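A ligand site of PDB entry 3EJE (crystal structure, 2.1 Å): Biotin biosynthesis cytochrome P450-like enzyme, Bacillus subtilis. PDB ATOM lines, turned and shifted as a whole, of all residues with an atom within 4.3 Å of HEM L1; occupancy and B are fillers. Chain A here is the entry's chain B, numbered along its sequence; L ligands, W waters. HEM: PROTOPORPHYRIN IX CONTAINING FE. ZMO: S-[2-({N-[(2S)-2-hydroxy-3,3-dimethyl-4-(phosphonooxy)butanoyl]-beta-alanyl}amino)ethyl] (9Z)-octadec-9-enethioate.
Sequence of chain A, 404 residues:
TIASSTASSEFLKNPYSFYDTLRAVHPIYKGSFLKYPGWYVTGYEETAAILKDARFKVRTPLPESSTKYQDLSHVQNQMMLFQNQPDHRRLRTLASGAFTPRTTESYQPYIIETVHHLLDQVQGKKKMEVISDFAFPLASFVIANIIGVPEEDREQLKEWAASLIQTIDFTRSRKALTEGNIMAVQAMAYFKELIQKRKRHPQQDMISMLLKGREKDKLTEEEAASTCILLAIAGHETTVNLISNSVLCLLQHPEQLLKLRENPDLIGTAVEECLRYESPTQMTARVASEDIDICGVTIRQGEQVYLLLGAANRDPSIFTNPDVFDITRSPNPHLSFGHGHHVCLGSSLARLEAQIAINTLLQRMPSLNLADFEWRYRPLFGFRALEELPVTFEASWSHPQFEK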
ATOM      1  N   LEU A  51      20.734  37.681 -28.041  1.00  0.00           N
ATOM      2  CA  LEU A  51      21.113  36.328 -27.639  1.00  0.00           C
ATOM      3  C   LEU A  51      20.061  35.287 -28.018  1.00  0.00           C
ATOM      4  O   LEU A  51      20.378  34.120 -28.259  1.00  0.00           O
ATOM      5  CB  LEU A  51      21.386  36.277 -26.125  1.00  0.00           C
ATOM      6  CG  LEU A  51      22.655  36.985 -25.648  1.00  0.00           C
ATOM      7  CD1 LEU A  51      22.637  37.156 -24.134  1.00  0.00           C
ATOM      8  CD2 LEU A  51      23.908  36.230 -26.091  1.00  0.00           C
ATOM      9  N   MET A  80      31.778  23.776 -28.751  1.00  0.00           N
ATOM     10  CA  MET A  80      30.349  24.059 -28.959  1.00  0.00           C
ATOM     11  C   MET A  80      30.021  25.541 -28.781  1.00  0.00           C
ATOM     12  O   MET A  80      29.051  26.037 -29.352  1.00  0.00           O
ATOM     13  CB  MET A  80      29.495  23.215 -28.006  1.00  0.00           C
ATOM     14  CG  MET A  80      29.506  23.681 -26.558  1.00  0.00           C
ATOM     15  SD  MET A  80      28.406  22.751 -25.485  1.00  0.00           S
ATOM     16  CE  MET A  80      29.515  21.455 -24.923  1.00  0.00           C
ATOM     17  N   LEU A  81      30.831  26.231 -27.989  1.00  0.00           N
ATOM     18  CA  LEU A  81      30.637  27.646 -27.691  1.00  0.00           C
ATOM     19  C   LEU A  81      30.765  28.508 -28.947  1.00  0.00           C
ATOM     20  O   LEU A  81      30.151  29.575 -29.039  1.00  0.00           O
ATOM     21  CB  LEU A  81      31.648  28.097 -26.638  1.00  0.00           C
ATOM     22  CG  LEU A  81      31.590  29.533 -26.107  1.00  0.00           C
ATOM     23  CD1 LEU A  81      30.328  29.770 -25.297  1.00  0.00           C
ATOM     24  CD2 LEU A  81      32.820  29.833 -25.282  1.00  0.00           C
ATOM     25  N   HIS A  88      26.264  22.556 -33.238  1.00  0.00           N
ATOM     26  CA  HIS A  88      26.091  23.012 -31.853  1.00  0.00           C
ATOM     27  C   HIS A  88      25.205  22.068 -31.038  1.00  0.00           C
ATOM     28  O   HIS A  88      25.601  21.622 -29.968  1.00  0.00           O
ATOM     29  CB  HIS A  88      25.516  24.438 -31.810  1.00  0.00           C
ATOM     30  CG  HIS A  88      25.102  24.864 -30.436  1.00  0.00           C
ATOM     31  ND1 HIS A  88      23.780  25.076 -30.083  1.00  0.00           N
ATOM     32  CD2 HIS A  88      25.827  25.074 -29.315  1.00  0.00           C
ATOM     33  CE1 HIS A  88      23.719  25.417 -28.815  1.00  0.00           C
ATOM     34  NE2 HIS A  88      24.951  25.426 -28.320  1.00  0.00           N
ATOM     35  N   ARG A  92      26.385  19.926 -27.822  1.00  0.00           N
ATOM     36  CA  ARG A  92      25.779  20.300 -26.542  1.00  0.00           C
ATOM     37  C   ARG A  92      25.020  19.142 -25.908  1.00  0.00           C
ATOM     38  O   ARG A  92      25.210  18.834 -24.732  1.00  0.00           O
ATOM     39  CB  ARG A  92      24.865  21.517 -26.715  1.00  0.00           C
ATOM     40  CG  ARG A  92      24.447  22.168 -25.404  1.00  0.00           C
ATOM     41  CD  ARG A  92      23.420  23.259 -25.629  1.00  0.00           C
ATOM     42  NE  ARG A  92      22.677  23.542 -24.402  1.00  0.00           N
ATOM     43  CZ  ARG A  92      22.998  24.489 -23.523  1.00  0.00           C
ATOM     44  NH1 ARG A  92      24.041  25.275 -23.737  1.00  0.00           N
ATOM     45  NH2 ARG A  92      22.266  24.650 -22.428  1.00  0.00           N
ATOM     46  N   PHE A  99      25.457  17.421 -16.591  1.00  0.00           N
ATOM     47  CA  PHE A  99      25.054  18.705 -15.997  1.00  0.00           C
ATOM     48  C   PHE A  99      23.546  18.845 -15.806  1.00  0.00           C
ATOM     49  O   PHE A  99      23.047  19.937 -15.526  1.00  0.00           O
ATOM     50  CB  PHE A  99      25.608  19.867 -16.831  1.00  0.00           C
ATOM     51  CG  PHE A  99      27.099  19.841 -16.983  1.00  0.00           C
ATOM     52  CD1 PHE A  99      27.929  20.264 -15.957  1.00  0.00           C
ATOM     53  CD2 PHE A  99      27.682  19.364 -18.155  1.00  0.00           C
ATOM     54  CE1 PHE A  99      29.312  20.225 -16.093  1.00  0.00           C
ATOM     55  CE2 PHE A  99      29.065  19.315 -18.295  1.00  0.00           C
ATOM     56  CZ  PHE A  99      29.875  19.745 -17.264  1.00  0.00           C
ATOM     57  N   ILE A 143      35.719  19.930 -10.950  1.00  0.00           N
ATOM     58  CA  ILE A 143      35.661  19.761 -12.410  1.00  0.00           C
ATOM     59  C   ILE A 143      36.588  18.651 -12.918  1.00  0.00           C
ATOM     60  O   ILE A 143      36.260  17.948 -13.875  1.00  0.00           O
ATOM     61  CB  ILE A 143      35.934  21.099 -13.155  1.00  0.00           C
ATOM     62  CG1 ILE A 143      35.345  21.041 -14.575  1.00  0.00           C
ATOM     63  CG2 ILE A 143      37.421  21.435 -13.200  1.00  0.00           C
ATOM     64  CD1 ILE A 143      33.839  20.853 -14.622  1.00  0.00           C
ATOM     65  N   LEU A 230      37.240  22.768 -22.916  1.00  0.00           N
ATOM     66  CA  LEU A 230      36.266  23.843 -22.691  1.00  0.00           C
ATOM     67  C   LEU A 230      35.706  23.797 -21.271  1.00  0.00           C
ATOM     68  O   LEU A 230      35.687  24.808 -20.568  1.00  0.00           O
ATOM     69  CB  LEU A 230      35.134  23.758 -23.723  1.00  0.00           C
ATOM     70  CG  LEU A 230      33.854  24.563 -23.466  1.00  0.00           C
ATOM     71  CD1 LEU A 230      34.128  26.063 -23.416  1.00  0.00           C
ATOM     72  CD2 LEU A 230      32.820  24.248 -24.525  1.00  0.00           C
ATOM     73  N   LEU A 231      35.245  22.615 -20.864  1.00  0.00           N
ATOM     74  CA  LEU A 231      34.650  22.438 -19.541  1.00  0.00           C
ATOM     75  C   LEU A 231      35.669  22.628 -18.420  1.00  0.00           C
ATOM     76  O   LEU A 231      35.336  23.152 -17.354  1.00  0.00           O
ATOM     77  CB  LEU A 231      33.973  21.071 -19.431  1.00  0.00           C
ATOM     78  CG  LEU A 231      32.769  20.843 -20.369  1.00  0.00           C
ATOM     79  CD1 LEU A 231      32.411  19.376 -20.427  1.00  0.00           C
ATOM     80  CD2 LEU A 231      31.571  21.661 -19.934  1.00  0.00           C
ATOM     81  N   ALA A 234      36.152  26.500 -18.158  1.00  0.00           N
ATOM     82  CA  ALA A 234      34.947  27.063 -17.559  1.00  0.00           C
ATOM     83  C   ALA A 234      34.851  26.716 -16.076  1.00  0.00           C
ATOM     84  O   ALA A 234      34.503  27.565 -15.248  1.00  0.00           O
ATOM     85  CB  ALA A 234      33.710  26.574 -18.300  1.00  0.00           C
ATOM     86  N   GLY A 235      35.176  25.463 -15.740  1.00  0.00           N
ATOM     87  CA  GLY A 235      35.144  24.993 -14.362  1.00  0.00           C
ATOM     88  C   GLY A 235      36.144  25.680 -13.458  1.00  0.00           C
ATOM     89  O   GLY A 235      35.875  25.910 -12.279  1.00  0.00           O
ATOM     90  N   THR A 238      35.716  30.762 -14.333  1.00  0.00           N
ATOM     91  CA  THR A 238      34.486  31.498 -14.026  1.00  0.00           C
ATOM     92  C   THR A 238      33.906  31.183 -12.652  1.00  0.00           C
ATOM     93  O   THR A 238      33.424  32.072 -11.958  1.00  0.00           O
ATOM     94  CB  THR A 238      33.400  31.297 -15.112  1.00  0.00           C
ATOM     95  OG1 THR A 238      33.186  29.895 -15.322  1.00  0.00           O
ATOM     96  CG2 THR A 238      33.824  31.944 -16.422  1.00  0.00           C
ATOM     97  N   THR A 239      33.946  29.900 -12.265  1.00  0.00           N
ATOM     98  CA  THR A 239      33.400  29.481 -10.970  1.00  0.00           C
ATOM     99  C   THR A 239      34.218  30.035  -9.808  1.00  0.00           C
ATOM    100  O   THR A 239      33.662  30.432  -8.782  1.00  0.00           O
ATOM    101  CB  THR A 239      33.301  27.940 -10.858  1.00  0.00           C
ATOM    102  OG1 THR A 239      32.612  27.423 -11.994  1.00  0.00           O
ATOM    103  CG2 THR A 239      32.540  27.547  -9.593  1.00  0.00           C
ATOM    104  N   LEU A 275      25.600  37.189  -8.657  1.00  0.00           N
ATOM    105  CA  LEU A 275      25.718  36.985 -10.098  1.00  0.00           C
ATOM    106  C   LEU A 275      25.331  38.231 -10.882  1.00  0.00           C
ATOM    107  O   LEU A 275      25.995  38.592 -11.859  1.00  0.00           O
ATOM    108  CB  LEU A 275      24.876  35.784 -10.539  1.00  0.00           C
ATOM    109  CG  LEU A 275      25.504  34.411 -10.334  1.00  0.00           C
ATOM    110  CD1 LEU A 275      24.438  33.330 -10.247  1.00  0.00           C
ATOM    111  CD2 LEU A 275      26.489  34.102 -11.444  1.00  0.00           C
ATOM    112  N   PRO A 280      30.809  37.284 -13.145  1.00  0.00           N
ATOM    113  CA  PRO A 280      32.085  36.674 -13.517  1.00  0.00           C
ATOM    114  C   PRO A 280      32.404  36.870 -15.013  1.00  0.00           C
ATOM    115  O   PRO A 280      33.542  37.163 -15.356  1.00  0.00           O
ATOM    116  CB  PRO A 280      31.874  35.187 -13.217  1.00  0.00           C
ATOM    117  CG  PRO A 280      30.845  35.178 -12.130  1.00  0.00           C
ATOM    118  CD  PRO A 280      29.927  36.321 -12.442  1.00  0.00           C
ATOM    119  N   THR A 281      31.392  36.716 -15.857  1.00  0.00           N
ATOM    120  CA  THR A 281      31.529  36.981 -17.285  1.00  0.00           C
ATOM    121  C   THR A 281      30.943  38.345 -17.623  1.00  0.00           C
ATOM    122  O   THR A 281      29.760  38.594 -17.392  1.00  0.00           O
ATOM    123  CB  THR A 281      30.830  35.888 -18.139  1.00  0.00           C
ATOM    124  OG1 THR A 281      31.425  34.620 -17.854  1.00  0.00           O
ATOM    125  CG2 THR A 281      30.970  36.195 -19.625  1.00  0.00           C
ATOM    126  N   THR A 284      30.067  38.621 -23.835  1.00  0.00           N
ATOM    127  CA  THR A 284      30.115  37.655 -24.925  1.00  0.00           C
ATOM    128  C   THR A 284      29.878  38.366 -26.250  1.00  0.00           C
ATOM    129  O   THR A 284      29.699  39.582 -26.282  1.00  0.00           O
ATOM    130  CB  THR A 284      29.138  36.471 -24.697  1.00  0.00           C
ATOM    131  OG1 THR A 284      29.400  35.447 -25.673  1.00  0.00           O
ATOM    132  CG2 THR A 284      27.682  36.917 -24.807  1.00  0.00           C
ATOM    133  N   ARG A 286      28.644  38.182 -30.701  1.00  0.00           N
ATOM    134  CA  ARG A 286      27.952  37.575 -31.837  1.00  0.00           C
ATOM    135  C   ARG A 286      28.342  38.282 -33.135  1.00  0.00           C
ATOM    136  O   ARG A 286      28.797  39.429 -33.107  1.00  0.00           O
ATOM    137  CB  ARG A 286      26.429  37.655 -31.642  1.00  0.00           C
ATOM    138  CG  ARG A 286      25.879  36.847 -30.468  1.00  0.00           C
ATOM    139  CD  ARG A 286      25.962  35.350 -30.727  1.00  0.00           C
ATOM    140  NE  ARG A 286      25.289  34.565 -29.696  1.00  0.00           N
ATOM    141  CZ  ARG A 286      25.858  34.151 -28.562  1.00  0.00           C
ATOM    142  NH1 ARG A 286      27.118  34.467 -28.286  1.00  0.00           N
ATOM    143  NH2 ARG A 286      25.158  33.420 -27.704  1.00  0.00           N
ATOM    144  N   LEU A 309      27.284  41.865 -20.453  1.00  0.00           N
ATOM    145  CA  LEU A 309      26.306  41.226 -19.561  1.00  0.00           C
ATOM    146  C   LEU A 309      26.221  41.915 -18.202  1.00  0.00           C
ATOM    147  O   LEU A 309      25.145  42.032 -17.622  1.00  0.00           O
ATOM    148  CB  LEU A 309      26.661  39.746 -19.369  1.00  0.00           C
ATOM    149  CG  LEU A 309      26.750  38.867 -20.622  1.00  0.00           C
ATOM    150  CD1 LEU A 309      27.248  37.490 -20.269  1.00  0.00           C
ATOM    151  CD2 LEU A 309      25.417  38.796 -21.352  1.00  0.00           C
ATOM    152  N   SER A 336      23.815  36.783 -16.470  1.00  0.00           N
ATOM    153  CA  SER A 336      25.188  36.390 -16.187  1.00  0.00           C
ATOM    154  C   SER A 336      25.555  35.041 -16.810  1.00  0.00           C
ATOM    155  O   SER A 336      26.721  34.793 -17.130  1.00  0.00           O
ATOM    156  CB  SER A 336      25.437  36.373 -14.676  1.00  0.00           C
ATOM    157  OG  SER A 336      25.262  37.669 -14.125  1.00  0.00           O
ATOM    158  N   PHE A 337      24.562  34.176 -16.981  1.00  0.00           N
ATOM    159  CA  PHE A 337      24.752  32.879 -17.614  1.00  0.00           C
ATOM    160  C   PHE A 337      24.363  32.897 -19.097  1.00  0.00           C
ATOM    161  O   PHE A 337      24.298  31.848 -19.754  1.00  0.00           O
ATOM    162  CB  PHE A 337      23.943  31.800 -16.877  1.00  0.00           C
ATOM    163  CG  PHE A 337      24.523  31.419 -15.546  1.00  0.00           C
ATOM    164  CD1 PHE A 337      23.803  31.629 -14.371  1.00  0.00           C
ATOM    165  CD2 PHE A 337      25.787  30.850 -15.454  1.00  0.00           C
ATOM    166  CE1 PHE A 337      24.325  31.263 -13.139  1.00  0.00           C
ATOM    167  CE2 PHE A 337      26.318  30.493 -14.218  1.00  0.00           C
ATOM    168  CZ  PHE A 337      25.587  30.702 -13.065  1.00  0.00           C
ATOM    169  N   GLY A 338      24.101  34.082 -19.622  1.00  0.00           N
ATOM    170  CA  GLY A 338      23.688  34.240 -21.007  1.00  0.00           C
ATOM    171  C   GLY A 338      22.205  33.998 -21.209  1.00  0.00           C
ATOM    172  O   GLY A 338      21.415  34.134 -20.267  1.00  0.00           O
ATOM    173  N   HIS A 341      20.142  29.756 -27.051  1.00  0.00           N
ATOM    174  CA  HIS A 341      20.658  28.428 -27.376  1.00  0.00           C
ATOM    175  C   HIS A 341      21.983  28.091 -26.708  1.00  0.00           C
ATOM    176  O   HIS A 341      22.257  26.925 -26.412  1.00  0.00           O
ATOM    177  CB  HIS A 341      20.768  28.252 -28.892  1.00  0.00           C
ATOM    178  CG  HIS A 341      19.464  27.998 -29.573  1.00  0.00           C
ATOM    179  ND1 HIS A 341      19.085  28.626 -30.731  1.00  0.00           N
ATOM    180  CD2 HIS A 341      18.432  27.175 -29.243  1.00  0.00           C
ATOM    181  CE1 HIS A 341      17.888  28.205 -31.103  1.00  0.00           C
ATOM    182  NE2 HIS A 341      17.466  27.323 -30.208  1.00  0.00           N
ATOM    183  N   HIS A 342      22.807  29.102 -26.464  1.00  0.00           N
ATOM    184  CA  HIS A 342      24.142  28.903 -25.908  1.00  0.00           C
ATOM    185  C   HIS A 342      24.196  29.151 -24.407  1.00  0.00           C
ATOM    186  O   HIS A 342      25.279  29.209 -23.825  1.00  0.00           O
ATOM    187  CB  HIS A 342      25.160  29.784 -26.635  1.00  0.00           C
ATOM    188  CG  HIS A 342      25.473  29.341 -28.029  1.00  0.00           C
ATOM    189  ND1 HIS A 342      26.451  28.407 -28.307  1.00  0.00           N
ATOM    190  CD2 HIS A 342      24.936  29.691 -29.211  1.00  0.00           C
ATOM    191  CE1 HIS A 342      26.507  28.209 -29.613  1.00  0.00           C
ATOM    192  NE2 HIS A 342      25.594  28.979 -30.185  1.00  0.00           N
ATOM    193  N   VAL A 343      23.032  29.274 -23.779  1.00  0.00           N
ATOM    194  CA  VAL A 343      22.950  29.534 -22.336  1.00  0.00           C
ATOM    195  C   VAL A 343      23.798  28.535 -21.546  1.00  0.00           C
ATOM    196  O   VAL A 343      23.858  27.351 -21.891  1.00  0.00           O
ATOM    197  CB  VAL A 343      21.476  29.537 -21.836  1.00  0.00           C
ATOM    198  CG1 VAL A 343      20.898  28.126 -21.805  1.00  0.00           C
ATOM    199  CG2 VAL A 343      21.375  30.192 -20.458  1.00  0.00           C
ATOM    200  N   CYS A 344      24.452  29.032 -20.507  1.00  0.00           N
ATOM    201  CA  CYS A 344      25.439  28.239 -19.775  1.00  0.00           C
ATOM    202  C   CYS A 344      24.991  26.812 -19.484  1.00  0.00           C
ATOM    203  O   CYS A 344      23.924  26.580 -18.926  1.00  0.00           O
ATOM    204  CB  CYS A 344      25.843  28.925 -18.474  1.00  0.00           C
ATOM    205  SG  CYS A 344      27.159  28.055 -17.604  1.00  0.00           S
ATOM    206  N   LEU A 345      25.833  25.859 -19.869  1.00  0.00           N
ATOM    207  CA  LEU A 345      25.558  24.440 -19.685  1.00  0.00           C
ATOM    208  C   LEU A 345      25.749  24.010 -18.232  1.00  0.00           C
ATOM    209  O   LEU A 345      25.035  23.132 -17.742  1.00  0.00           O
ATOM    210  CB  LEU A 345      26.462  23.609 -20.601  1.00  0.00           C
ATOM    211  CG  LEU A 345      26.190  22.115 -20.750  1.00  0.00           C
ATOM    212  CD1 LEU A 345      24.795  21.851 -21.312  1.00  0.00           C
ATOM    213  CD2 LEU A 345      27.261  21.473 -21.623  1.00  0.00           C
ATOM    214  N   GLY A 346      26.698  24.638 -17.545  1.00  0.00           N
ATOM    215  CA  GLY A 346      27.051  24.241 -16.184  1.00  0.00           C
ATOM    216  C   GLY A 346      26.551  25.186 -15.098  1.00  0.00           C
ATOM    217  O   GLY A 346      27.145  25.259 -14.010  1.00  0.00           O
ATOM    218  N   LEU A 349      25.707  23.582 -11.665  1.00  0.00           N
ATOM    219  CA  LEU A 349      26.919  23.199 -10.940  1.00  0.00           C
ATOM    220  C   LEU A 349      27.601  24.415 -10.326  1.00  0.00           C
ATOM    221  O   LEU A 349      28.008  24.382  -9.158  1.00  0.00           O
ATOM    222  CB  LEU A 349      27.894  22.469 -11.869  1.00  0.00           C
ATOM    223  CG  LEU A 349      29.280  22.140 -11.317  1.00  0.00           C
ATOM    224  CD1 LEU A 349      29.196  21.161 -10.160  1.00  0.00           C
ATOM    225  CD2 LEU A 349      30.176  21.594 -12.414  1.00  0.00           C
ATOM    226  N   ALA A 350      27.713  25.489 -11.098  1.00  0.00           N
ATOM    227  CA  ALA A 350      28.311  26.736 -10.639  1.00  0.00           C
ATOM    228  C   ALA A 350      27.573  27.284  -9.423  1.00  0.00           C
ATOM    229  O   ALA A 350      28.201  27.686  -8.442  1.00  0.00           O
ATOM    230  CB  ALA A 350      28.332  27.762 -11.764  1.00  0.00           C
HETATM  231  CHA HEM L   1      28.213  28.931 -21.809  1.00  0.00           C
HETATM  232  CHB HEM L   1      30.144  25.345 -19.174  1.00  0.00           C
HETATM  233  CHC HEM L   1      30.372  28.272 -15.299  1.00  0.00           C
HETATM  234  CHD HEM L   1      28.866  31.995 -18.026  1.00  0.00           C
HETATM  235  C1A HEM L   1      28.758  27.715 -21.458  1.00  0.00           C
HETATM  236  C2A HEM L   1      29.005  26.593 -22.335  1.00  0.00           C
HETATM  237  C3A HEM L   1      29.536  25.607 -21.603  1.00  0.00           C
HETATM  238  C4A HEM L   1      29.643  26.065 -20.238  1.00  0.00           C
HETATM  239  CMA HEM L   1      29.956  24.206 -22.101  1.00  0.00           C
HETATM  240  CAA HEM L   1      28.700  26.556 -23.856  1.00  0.00           C
HETATM  241  CBA HEM L   1      27.225  26.234 -24.054  1.00  0.00           C
HETATM  242  CGA HEM L   1      26.846  26.275 -25.515  1.00  0.00           C
HETATM  243  O1A HEM L   1      25.773  25.725 -25.865  1.00  0.00           O
HETATM  244  O2A HEM L   1      27.614  26.840 -26.331  1.00  0.00           O
HETATM  245  C1B HEM L   1      30.334  25.816 -17.891  1.00  0.00           C
HETATM  246  C2B HEM L   1      30.766  25.022 -16.756  1.00  0.00           C
HETATM  247  C3B HEM L   1      30.830  25.827 -15.694  1.00  0.00           C
HETATM  248  C4B HEM L   1      30.443  27.160 -16.105  1.00  0.00           C
HETATM  249  CMB HEM L   1      31.087  23.510 -16.791  1.00  0.00           C
HETATM  250  CAB HEM L   1      31.229  25.433 -14.247  1.00  0.00           C
HETATM  251  CBB HEM L   1      31.937  24.327 -14.005  1.00  0.00           C
HETATM  252  C1C HEM L   1      29.972  29.537 -15.687  1.00  0.00           C
HETATM  253  C2C HEM L   1      29.869  30.708 -14.825  1.00  0.00           C
HETATM  254  C3C HEM L   1      29.444  31.725 -15.586  1.00  0.00           C
HETATM  255  C4C HEM L   1      29.280  31.249 -16.942  1.00  0.00           C
HETATM  256  CMC HEM L   1      30.184  30.741 -13.318  1.00  0.00           C
HETATM  257  CAC HEM L   1      29.196  33.187 -15.145  1.00  0.00           C
HETATM  258  CBC HEM L   1      28.312  33.480 -14.191  1.00  0.00           C
HETATM  259  C1D HEM L   1      28.507  31.522 -19.278  1.00  0.00           C
HETATM  260  C2D HEM L   1      27.901  32.313 -20.316  1.00  0.00           C
HETATM  261  C3D HEM L   1      27.700  31.359 -21.496  1.00  0.00           C
HETATM  262  C4D HEM L   1      28.205  30.085 -21.057  1.00  0.00           C
HETATM  263  CMD HEM L   1      27.551  33.822 -20.257  1.00  0.00           C
HETATM  264  CAD HEM L   1      27.089  31.706 -22.874  1.00  0.00           C
HETATM  265  CBD HEM L   1      28.054  32.589 -23.651  1.00  0.00           C
HETATM  266  CGD HEM L   1      27.487  32.899 -25.020  1.00  0.00           C
HETATM  267  O1D HEM L   1      28.285  33.298 -25.902  1.00  0.00           O
HETATM  268  O2D HEM L   1      26.246  32.773 -25.224  1.00  0.00           O
HETATM  269  NA  HEM L   1      29.161  27.356 -20.186  1.00  0.00           N
HETATM  270  NB  HEM L   1      30.150  27.108 -17.466  1.00  0.00           N
HETATM  271  NC  HEM L   1      29.617  29.914 -16.967  1.00  0.00           N
HETATM  272  ND  HEM L   1      28.669  30.215 -19.743  1.00  0.00           N
HETATM  273 FE   HEM L   1      29.250  28.602 -18.515  1.00  0.00          FE
HETATM  274  O23 ZMO L   2      37.941  37.158 -39.382  1.00  0.00           O
HETATM  275  P24 ZMO L   2      37.686  38.701 -38.796  1.00  0.00           P
HETATM  276  O26 ZMO L   2      36.670  39.728 -39.654  1.00  0.00           O
HETATM  277  O27 ZMO L   2      37.810  38.969 -36.999  1.00  0.00           O
HETATM  278  C28 ZMO L   2      36.713  38.604 -36.167  1.00  0.00           C
HETATM  279  C29 ZMO L   2      37.225  38.092 -34.828  1.00  0.00           C
HETATM  280  C31 ZMO L   2      38.156  36.915 -35.077  1.00  0.00           C
HETATM  281  C30 ZMO L   2      36.048  37.613 -34.000  1.00  0.00           C
HETATM  282  C32 ZMO L   2      38.002  39.212 -34.127  1.00  0.00           C
HETATM  283  O33 ZMO L   2      39.016  38.674 -33.255  1.00  0.00           O
HETATM  284  C34 ZMO L   2      37.064  40.092 -33.351  1.00  0.00           C
HETATM  285  O35 ZMO L   2      36.195  40.840 -34.030  1.00  0.00           O
HETATM  286  N36 ZMO L   2      37.078  40.143 -32.083  1.00  0.00           N
HETATM  287  C37 ZMO L   2      37.943  39.399 -31.175  1.00  0.00           C
HETATM  288  C38 ZMO L   2      37.441  39.714 -29.768  1.00  0.00           C
HETATM  289  C39 ZMO L   2      36.333  38.772 -29.389  1.00  0.00           C
HETATM  290  O40 ZMO L   2      35.263  38.638 -30.171  1.00  0.00           O
HETATM  291  N41 ZMO L   2      36.406  38.123 -28.307  1.00  0.00           N
HETATM  292  C42 ZMO L   2      35.429  37.185 -27.772  1.00  0.00           C
HETATM  293  C43 ZMO L   2      34.593  37.985 -26.789  1.00  0.00           C
HETATM  294  S1  ZMO L   2      33.992  36.919 -25.515  1.00  0.00           S
HETATM  295  C1  ZMO L   2      33.380  35.414 -26.218  1.00  0.00           C
HETATM  296  O1  ZMO L   2      32.880  35.428 -27.442  1.00  0.00           O
HETATM  297  C2  ZMO L   2      33.086  34.224 -25.304  1.00  0.00           C
HETATM  298  C3  ZMO L   2      32.412  34.692 -24.013  1.00  0.00           C
HETATM  299  C4  ZMO L   2      31.794  33.521 -23.255  1.00  0.00           C
HETATM  300  C5  ZMO L   2      32.531  33.285 -21.947  1.00  0.00           C
HETATM  301  C6  ZMO L   2      31.627  32.588 -20.935  1.00  0.00           C
HETATM  302  C7  ZMO L   2      32.010  31.119 -20.762  1.00  0.00           C
HETATM  303  C8  ZMO L   2      33.455  30.962 -20.298  1.00  0.00           C
HETATM  304  C9  ZMO L   2      33.848  29.492 -20.275  1.00  0.00           C
HETATM  305  C10 ZMO L   2      34.822  29.006 -21.045  1.00  0.00           C
HETATM  306  C11 ZMO L   2      35.613  29.872 -22.025  1.00  0.00           C
HETATM  307  C12 ZMO L   2      36.831  29.106 -22.537  1.00  0.00           C
HETATM  308  C13 ZMO L   2      37.219  29.518 -23.942  1.00  0.00           C
HETATM  309  C14 ZMO L   2      38.711  29.305 -24.167  1.00  0.00           C
HETATM  310  C15 ZMO L   2      38.989  28.624 -25.499  1.00  0.00           C
HETATM  311  C16 ZMO L   2      40.474  28.397 -25.698  1.00  0.00           C
HETATM  312  O   HOH W   1      23.854  32.781 -24.173  1.00  0.00           O
HETATM  313  O   HOH W   2      30.301  32.363 -28.007  1.00  0.00           O
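O1A of HEM L1 sits at hydrogen-bond distance from NE2 of His 88. O2D of HEM L1 lies within salt-bridge range of NH2 of Arg 286 (2.8 Å). ND1 of His 342 lies within hydrogen-bond range of O2A of HEM L1, 2.8 Å away. The side-chain hydroxyl of Thr 284 lies within hydrogen-bond range of an oxygen (O1D) of HEM L1, at 2.4 Å. The guanidinium group of Arg 92 lies within salt-bridge range of an oxygen (O1A) of HEM L1 (2.8 Å). An iron atom (FE) of HEM L1 is bound by the side-chain sulfur of Cys 344 (2.3 Å).
The backbone carbonyl oxygen of Leu 275 lies within hydrogen-bond range of the side-chain hydroxyl of Ser 336 (2.6 Å). A ring nitrogen (NE2) of His 88 is in hydrogen-bond range of a ring nitrogen (ND1) of His 342, 3.3 Å away. The side-chain sulfur (SG) of Cys 344 sits close to the backbone NH (N) of Gly 346 (3.4 Å). The backbone NH (N) of Cys 344 sits at hydrogen-bond distance from the backbone carbonyl oxygen (O) of Phe 337, 2.9 Å away. The backbone carbonyl oxygen (O) of Val 343 sits at hydrogen-bond distance from the guanidinium group (NH1) of Arg 92 (2.8 Å). The backbone carbonyl oxygen (O) of Ala 234 is in hydrogen-bond range of the side-chain hydroxyl (OG1) of Thr 238.
The backbone carbonyl oxygen (O) of Met 80 sits close to an oxygen (O2A) of HEM L1 (3.4 Å). Leu 81 touches HEM L1. Phe 99 touches HEM L1. Leu 230 touches HEM L1. CD2 of Leu 231 touches CMB of HEM L1 (3.7 Å). Ala 234 touches HEM L1 (CB to C1B, 3.5 Å). Gly 235 touches HEM L1 (CA to CBB, 3.3 Å). OG1 of Thr 238 touches CHC of HEM L1, at 3.2 Å. Thr 239 touches HEM L1 (OG1 to CAB, 3.3 Å). Leu 275 touches HEM L1 (CD2 to CBC, 3.4 Å). Pro 280 touches HEM L1. Thr 281 touches HEM L1 (OG1 to CHD, 3.7 Å). CD1 of Leu 309 touches CMD of HEM L1, at 3.7 Å. Ser 336 touches HEM L1 (O to CMD, 3.4 Å). Phe 337 touches HEM L1 (C to CMD, 3.5 Å). Gly 338 touches HEM L1. His 341 touches HEM L1 (O to O1A, 3.8 Å). N of Leu 345 touches NA of HEM L1, at 3.7 Å. N of Gly 346 touches C1B of HEM L1, 3.8 Å away. CD2 of Leu 349 touches CBB of HEM L1, 3.6 Å away. CB of Ala 350 touches CMC of HEM L1, at 3.8 Å. Hydrophobic or aromatic side chains that line HEM L1: Met 80, Leu 81, His 88, Phe 99, Leu 230, Leu 231, Ala 234, Leu 275, Pro 280, Leu 309, Phe 337, His 342, Leu 345, Leu 349 and Ala 350.
Water W2 lies within hydrogen-bond range of the backbone carbonyl oxygen of Leu 81 (3.0 Å) and an oxygen (O1D) of HEM L1 (3.1 Å).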
